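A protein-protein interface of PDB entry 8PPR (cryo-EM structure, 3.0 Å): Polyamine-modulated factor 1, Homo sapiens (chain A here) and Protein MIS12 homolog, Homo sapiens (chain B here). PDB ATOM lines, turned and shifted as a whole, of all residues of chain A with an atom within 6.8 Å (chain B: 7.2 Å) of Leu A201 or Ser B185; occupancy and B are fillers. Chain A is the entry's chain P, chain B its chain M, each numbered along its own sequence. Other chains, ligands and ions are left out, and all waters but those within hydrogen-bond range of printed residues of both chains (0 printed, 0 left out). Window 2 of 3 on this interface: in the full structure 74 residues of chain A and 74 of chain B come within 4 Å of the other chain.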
ATOM      1  N   GLU A 196     -19.929   0.092   3.767  1.00  0.00           N
ATOM      2  CA  GLU A 196     -19.589   0.282   2.363  1.00  0.00           C
ATOM      3  C   GLU A 196     -18.936  -0.966   1.785  1.00  0.00           C
ATOM      4  O   GLU A 196     -19.240  -1.373   0.659  1.00  0.00           O
ATOM      5  CB  GLU A 196     -18.669   1.491   2.206  1.00  0.00           C
ATOM      6  CG  GLU A 196     -18.280   1.779   0.770  1.00  0.00           C
ATOM      7  CD  GLU A 196     -19.477   2.096  -0.105  1.00  0.00           C
ATOM      8  OE1 GLU A 196     -20.475   2.637   0.417  1.00  0.00           O
ATOM      9  OE2 GLU A 196     -19.421   1.798  -1.316  1.00  0.00           O
ATOM     10  N   LEU A 197     -18.032  -1.584   2.545  1.00  0.00           N
ATOM     11  CA  LEU A 197     -17.406  -2.821   2.095  1.00  0.00           C
ATOM     12  C   LEU A 197     -18.439  -3.927   1.934  1.00  0.00           C
ATOM     13  O   LEU A 197     -18.394  -4.695   0.965  1.00  0.00           O
ATOM     14  CB  LEU A 197     -16.317  -3.244   3.076  1.00  0.00           C
ATOM     15  CG  LEU A 197     -15.528  -4.495   2.695  1.00  0.00           C
ATOM     16  CD1 LEU A 197     -15.070  -4.414   1.248  1.00  0.00           C
ATOM     17  CD2 LEU A 197     -14.341  -4.676   3.626  1.00  0.00           C
ATOM     18  N   VAL A 198     -19.373  -4.027   2.881  1.00  0.00           N
ATOM     19  CA  VAL A 198     -20.440  -5.018   2.771  1.00  0.00           C
ATOM     20  C   VAL A 198     -21.253  -4.778   1.507  1.00  0.00           C
ATOM     21  O   VAL A 198     -21.638  -5.721   0.807  1.00  0.00           O
ATOM     22  CB  VAL A 198     -21.323  -4.991   4.031  1.00  0.00           C
ATOM     23  CG1 VAL A 198     -22.578  -5.822   3.823  1.00  0.00           C
ATOM     24  CG2 VAL A 198     -20.543  -5.494   5.233  1.00  0.00           C
ATOM     25  N   ALA A 199     -21.518  -3.510   1.193  1.00  0.00           N
ATOM     26  CA  ALA A 199     -22.226  -3.185  -0.041  1.00  0.00           C
ATOM     27  C   ALA A 199     -21.418  -3.604  -1.262  1.00  0.00           C
ATOM     28  O   ALA A 199     -21.975  -4.116  -2.241  1.00  0.00           O
ATOM     29  CB  ALA A 199     -22.537  -1.691  -0.090  1.00  0.00           C
ATOM     30  N   VAL A 200     -20.102  -3.392  -1.224  1.00  0.00           N
ATOM     31  CA  VAL A 200     -19.250  -3.796  -2.338  1.00  0.00           C
ATOM     32  C   VAL A 200     -19.281  -5.309  -2.507  1.00  0.00           C
ATOM     33  O   VAL A 200     -19.448  -5.824  -3.617  1.00  0.00           O
ATOM     34  CB  VAL A 200     -17.815  -3.283  -2.126  1.00  0.00           C
ATOM     35  CG1 VAL A 200     -16.876  -3.893  -3.155  1.00  0.00           C
ATOM     36  CG2 VAL A 200     -17.778  -1.767  -2.200  1.00  0.00           C
ATOM     37  N   LEU A 201     -19.133  -6.041  -1.405  1.00  0.00           N
ATOM     38  CA  LEU A 201     -19.159  -7.501  -1.429  1.00  0.00           C
ATOM     39  C   LEU A 201     -20.569  -7.946  -1.055  1.00  0.00           C
ATOM     40  O   LEU A 201     -20.853  -8.343   0.074  1.00  0.00           O
ATOM     41  CB  LEU A 201     -18.109  -8.073  -0.485  1.00  0.00           C
ATOM     42  CG  LEU A 201     -16.740  -7.398  -0.554  1.00  0.00           C
ATOM     43  CD1 LEU A 201     -15.797  -7.995   0.477  1.00  0.00           C
ATOM     44  CD2 LEU A 201     -16.155  -7.513  -1.953  1.00  0.00           C
ATOM     45  N   ARG A 202     -21.460  -7.876  -2.033  1.00  0.00           N
ATOM     46  CA  ARG A 202     -22.866  -8.176  -1.828  1.00  0.00           C
ATOM     47  C   ARG A 202     -23.154  -9.642  -2.122  1.00  0.00           C
ATOM     48  O   ARG A 202     -22.421 -10.317  -2.848  1.00  0.00           O
ATOM     49  CB  ARG A 202     -23.735  -7.284  -2.712  1.00  0.00           C
ATOM     50  CG  ARG A 202     -23.660  -7.643  -4.178  1.00  0.00           C
ATOM     51  CD  ARG A 202     -24.059  -6.469  -5.045  1.00  0.00           C
ATOM     52  NE  ARG A 202     -22.908  -5.630  -5.354  1.00  0.00           N
ATOM     53  CZ  ARG A 202     -21.940  -5.960  -6.199  1.00  0.00           C
ATOM     54  NH1 ARG A 202     -21.958  -7.108  -6.857  1.00  0.00           N
ATOM     55  NH2 ARG A 202     -20.928  -5.118  -6.388  1.00  0.00           N
ATOM     56  N   GLU A 203     -24.245 -10.126  -1.537  1.00  0.00           N
ATOM     57  CA  GLU A 203     -24.670 -11.494  -1.742  1.00  0.00           C
ATOM     58  C   GLU A 203     -25.190 -11.675  -3.165  1.00  0.00           C
ATOM     59  O   GLU A 203     -25.616 -10.712  -3.808  1.00  0.00           O
ATOM     60  CB  GLU A 203     -25.748 -11.857  -0.724  1.00  0.00           C
ATOM     61  CG  GLU A 203     -25.397 -11.441   0.696  1.00  0.00           C
ATOM     62  CD  GLU A 203     -26.398 -11.933   1.720  1.00  0.00           C
ATOM     63  OE1 GLU A 203     -27.255 -12.766   1.363  1.00  0.00           O
ATOM     64  OE2 GLU A 203     -26.324 -11.490   2.886  1.00  0.00           O
ATOM     65  N   LEU B 178      -9.375   0.485   5.698  1.00  0.00           N
ATOM     66  CA  LEU B 178     -10.679   0.038   5.228  1.00  0.00           C
ATOM     67  C   LEU B 178     -11.045   0.704   3.911  1.00  0.00           C
ATOM     68  O   LEU B 178     -11.613   0.062   3.023  1.00  0.00           O
ATOM     69  CB  LEU B 178     -11.741   0.328   6.286  1.00  0.00           C
ATOM     70  CG  LEU B 178     -11.686  -0.522   7.556  1.00  0.00           C
ATOM     71  CD1 LEU B 178     -12.755  -0.076   8.543  1.00  0.00           C
ATOM     72  CD2 LEU B 178     -11.829  -1.997   7.226  1.00  0.00           C
ATOM     73  N   VAL B 179     -10.737   1.994   3.771  1.00  0.00           N
ATOM     74  CA  VAL B 179     -11.056   2.696   2.532  1.00  0.00           C
ATOM     75  C   VAL B 179     -10.287   2.095   1.360  1.00  0.00           C
ATOM     76  O   VAL B 179     -10.853   1.838   0.287  1.00  0.00           O
ATOM     77  CB  VAL B 179     -10.769   4.198   2.686  1.00  0.00           C
ATOM     78  CG1 VAL B 179     -10.837   4.892   1.339  1.00  0.00           C
ATOM     79  CG2 VAL B 179     -11.748   4.826   3.664  1.00  0.00           C
ATOM     80  N   SER B 180      -8.987   1.858   1.550  1.00  0.00           N
ATOM     81  CA  SER B 180      -8.186   1.252   0.494  1.00  0.00           C
ATOM     82  C   SER B 180      -8.687  -0.146   0.165  1.00  0.00           C
ATOM     83  O   SER B 180      -8.741  -0.536  -1.009  1.00  0.00           O
ATOM     84  CB  SER B 180      -6.717   1.210   0.907  1.00  0.00           C
ATOM     85  OG  SER B 180      -5.972   0.381   0.033  1.00  0.00           O
ATOM     86  N   LEU B 181      -9.056  -0.915   1.190  1.00  0.00           N
ATOM     87  CA  LEU B 181      -9.584  -2.252   0.954  1.00  0.00           C
ATOM     88  C   LEU B 181     -10.886  -2.197   0.169  1.00  0.00           C
ATOM     89  O   LEU B 181     -11.122  -3.032  -0.706  1.00  0.00           O
ATOM     90  CB  LEU B 181      -9.782  -2.978   2.282  1.00  0.00           C
ATOM     91  CG  LEU B 181      -8.492  -3.473   2.938  1.00  0.00           C
ATOM     92  CD1 LEU B 181      -8.780  -4.105   4.289  1.00  0.00           C
ATOM     93  CD2 LEU B 181      -7.772  -4.450   2.024  1.00  0.00           C
ATOM     94  N   VAL B 182     -11.742  -1.219   0.466  1.00  0.00           N
ATOM     95  CA  VAL B 182     -13.002  -1.079  -0.262  1.00  0.00           C
ATOM     96  C   VAL B 182     -12.732  -0.759  -1.726  1.00  0.00           C
ATOM     97  O   VAL B 182     -13.347  -1.337  -2.634  1.00  0.00           O
ATOM     98  CB  VAL B 182     -13.880   0.001   0.395  1.00  0.00           C
ATOM     99  CG1 VAL B 182     -14.968   0.459  -0.564  1.00  0.00           C
ATOM    100  CG2 VAL B 182     -14.485  -0.519   1.684  1.00  0.00           C
ATOM    101  N   GLN B 183     -11.812   0.174  -1.976  1.00  0.00           N
ATOM    102  CA  GLN B 183     -11.486   0.539  -3.350  1.00  0.00           C
ATOM    103  C   GLN B 183     -10.934  -0.657  -4.115  1.00  0.00           C
ATOM    104  O   GLN B 183     -11.341  -0.934  -5.254  1.00  0.00           O
ATOM    105  CB  GLN B 183     -10.480   1.687  -3.350  1.00  0.00           C
ATOM    106  CG  GLN B 183     -11.035   2.983  -2.798  1.00  0.00           C
ATOM    107  CD  GLN B 183      -9.946   3.974  -2.455  1.00  0.00           C
ATOM    108  OE1 GLN B 183      -8.761   3.697  -2.637  1.00  0.00           O
ATOM    109  NE2 GLN B 183     -10.341   5.138  -1.954  1.00  0.00           N
ATOM    110  N   ASN B 184     -10.015  -1.392  -3.490  1.00  0.00           N
ATOM    111  CA  ASN B 184      -9.434  -2.558  -4.138  1.00  0.00           C
ATOM    112  C   ASN B 184     -10.469  -3.652  -4.346  1.00  0.00           C
ATOM    113  O   ASN B 184     -10.419  -4.366  -5.349  1.00  0.00           O
ATOM    114  CB  ASN B 184      -8.262  -3.077  -3.312  1.00  0.00           C
ATOM    115  CG  ASN B 184      -7.064  -2.158  -3.366  1.00  0.00           C
ATOM    116  OD1 ASN B 184      -6.956  -1.317  -4.259  1.00  0.00           O
ATOM    117  ND2 ASN B 184      -6.158  -2.306  -2.408  1.00  0.00           N
ATOM    118  N   SER B 185     -11.412  -3.796  -3.413  1.00  0.00           N
ATOM    119  CA  SER B 185     -12.477  -4.777  -3.573  1.00  0.00           C
ATOM    120  C   SER B 185     -13.371  -4.423  -4.750  1.00  0.00           C
ATOM    121  O   SER B 185     -13.787  -5.307  -5.504  1.00  0.00           O
ATOM    122  CB  SER B 185     -13.295  -4.874  -2.287  1.00  0.00           C
ATOM    123  OG  SER B 185     -12.575  -5.559  -1.279  1.00  0.00           O
ATOM    124  N   ARG B 186     -13.685  -3.139  -4.918  1.00  0.00           N
ATOM    125  CA  ARG B 186     -14.464  -2.725  -6.081  1.00  0.00           C
ATOM    126  C   ARG B 186     -13.709  -3.008  -7.373  1.00  0.00           C
ATOM    127  O   ARG B 186     -14.288  -3.502  -8.352  1.00  0.00           O
ATOM    128  CB  ARG B 186     -14.809  -1.242  -5.979  1.00  0.00           C
ATOM    129  CG  ARG B 186     -15.816  -0.772  -7.011  1.00  0.00           C
ATOM    130  CD  ARG B 186     -16.227   0.663  -6.744  1.00  0.00           C
ATOM    131  NE  ARG B 186     -17.064   0.774  -5.556  1.00  0.00           N
ATOM    132  CZ  ARG B 186     -16.661   1.298  -4.406  1.00  0.00           C
ATOM    133  NH1 ARG B 186     -15.431   1.759  -4.250  1.00  0.00           N
ATOM    134  NH2 ARG B 186     -17.513   1.358  -3.388  1.00  0.00           N
ATOM    135  N   LYS B 187     -12.410  -2.704  -7.392  1.00  0.00           N
ATOM    136  CA  LYS B 187     -11.605  -2.979  -8.575  1.00  0.00           C
ATOM    137  C   LYS B 187     -11.585  -4.470  -8.890  1.00  0.00           C
ATOM    138  O   LYS B 187     -11.741  -4.882 -10.048  1.00  0.00           O
ATOM    139  CB  LYS B 187     -10.187  -2.455  -8.363  1.00  0.00           C
ATOM    140  CG  LYS B 187      -9.293  -2.562  -9.576  1.00  0.00           C
ATOM    141  CD  LYS B 187      -8.254  -1.461  -9.556  1.00  0.00           C
ATOM    142  CE  LYS B 187      -7.398  -1.553  -8.305  1.00  0.00           C
ATOM    143  NZ  LYS B 187      -6.087  -0.872  -8.477  1.00  0.00           N
ATOM    144  N   LEU B 188     -11.401  -5.297  -7.861  1.00  0.00           N
ATOM    145  CA  LEU B 188     -11.379  -6.739  -8.058  1.00  0.00           C
ATOM    146  C   LEU B 188     -12.740  -7.264  -8.485  1.00  0.00           C
ATOM    147  O   LEU B 188     -12.815  -8.224  -9.251  1.00  0.00           O
ATOM    148  CB  LEU B 188     -10.918  -7.435  -6.779  1.00  0.00           C
ATOM    149  CG  LEU B 188     -10.757  -8.952  -6.878  1.00  0.00           C
ATOM    150  CD1 LEU B 188      -9.900  -9.317  -8.078  1.00  0.00           C
ATOM    151  CD2 LEU B 188     -10.156  -9.511  -5.601  1.00  0.00           C
ATOM    152  N   GLN B 189     -13.821  -6.657  -7.998  1.00  0.00           N
ATOM    153  CA  GLN B 189     -15.149  -7.048  -8.451  1.00  0.00           C
ATOM    154  C   GLN B 189     -15.327  -6.745  -9.930  1.00  0.00           C
ATOM    155  O   GLN B 189     -15.893  -7.555 -10.672  1.00  0.00           O
ATOM    156  CB  GLN B 189     -16.216  -6.335  -7.625  1.00  0.00           C
ATOM    157  CG  GLN B 189     -17.581  -6.988  -7.705  1.00  0.00           C
ATOM    158  CD  GLN B 189     -17.566  -8.415  -7.200  1.00  0.00           C
ATOM    159  OE1 GLN B 189     -17.722  -9.360  -7.972  1.00  0.00           O
ATOM    160  NE2 GLN B 189     -17.375  -8.579  -5.896  1.00  0.00           N
ATOM    161  N   ASN B 190     -14.847  -5.583 -10.375  1.00  0.00           N
ATOM    162  CA  ASN B 190     -14.898  -5.266 -11.800  1.00  0.00           C
ATOM    163  C   ASN B 190     -14.092  -6.273 -12.609  1.00  0.00           C
ATOM    164  O   ASN B 190     -14.541  -6.750 -13.664  1.00  0.00           O
ATOM    165  CB  ASN B 190     -14.372  -3.853 -12.034  1.00  0.00           C
ATOM    166  CG  ASN B 190     -15.318  -2.792 -11.522  1.00  0.00           C
ATOM    167  OD1 ASN B 190     -16.535  -2.964 -11.552  1.00  0.00           O
ATOM    168  ND2 ASN B 190     -14.762  -1.689 -11.036  1.00  0.00           N
ATOM    169  N   ILE B 191     -12.897  -6.609 -12.122  1.00  0.00           N
ATOM    170  CA  ILE B 191     -12.051  -7.580 -12.810  1.00  0.00           C
ATOM    171  C   ILE B 191     -12.747  -8.931 -12.884  1.00  0.00           C
ATOM    172  O   ILE B 191     -12.736  -9.598 -13.923  1.00  0.00           O
ATOM    173  CB  ILE B 191     -10.688  -7.682 -12.104  1.00  0.00           C
ATOM    174  CG1 ILE B 191      -9.897  -6.388 -12.292  1.00  0.00           C
ATOM    175  CG2 ILE B 191      -9.903  -8.872 -12.629  1.00  0.00           C
ATOM    176  CD1 ILE B 191      -8.610  -6.347 -11.502  1.00  0.00           C
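Among the printed residues, merely in contact across the chains: Glu A196 with Val B182, Leu A197 with Val B182, Leu A197 with Ser B185, Val A200 with Val B182, Val A200 with Ser B185, Val A200 with Arg B186 and Leu A201 with Ser B185.
NH2 of Arg B186 lies within salt-bridge range of OE2 of Glu A196 (2.9 Å).
Of the 14 printed residues of chain B, 3 touch a printed residue of chain A. Printed residues of chain B that touch a printed residue of chain A: Val B182, Ser B185 and Arg B186. Hydrophobic or aromatic side chains of chain A within 4 Å of the printed part of chain B: Leu A197, Val A200 and Leu A201. Among the printed residues, 8 pairs touch across the chains.
Of chain B, only Ser B185 (3.9 Å) comes within 4 Å of Leu A201. Of chain A, only Leu A197, Val A200 and Leu A201 come within 4 Å of Ser B185. Printed residues of chain B within 4 Å of Val A200: Val B182 (3.9 Å), Ser B185 (3.8 Å) and Arg B186 (3.4 Å). Of the printed residues of chain A, Arg B186 touches Glu A196 (2.9 Å) and Val A200 (3.4 Å). Of the printed residues of chain A, Val B182 touches Glu A196 (3.8 Å), Leu A197 (3.6 Å) and Val A200 (3.9 Å). Printed residues of chain B within 4 Å of Leu A197: Val B182 (3.6 Å) and Ser B185 (3.7 Å). Printed residues of chain B within 4 Å of Glu A196: Val B182 (3.8 Å) and Arg B186 (2.9 Å). Asn B190 touches none of the printed residues of chain A. Val B179 touches none of the printed residues of chain A. The nearest printed residue of chain A that does not touch Ser B185 is Arg A202 (7.2 Å). The nearest printed residue of chain B that does not touch Leu A197 is Leu B181 (4.6 Å).
The backbone carbonyl oxygen (O) of Arg B186 sits at hydrogen-bond distance from the side-chain amide nitrogen (ND2) of Asn B190. The guanidinium group (NH2) of Arg A202 lies within hydrogen-bond range of the backbone carbonyl oxygen (O) of Val A200, at 3.2 Å. The backbone carbonyl oxygen of Leu B181 lies within hydrogen-bond range of the side-chain hydroxyl of Ser B185 (3.0 Å).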
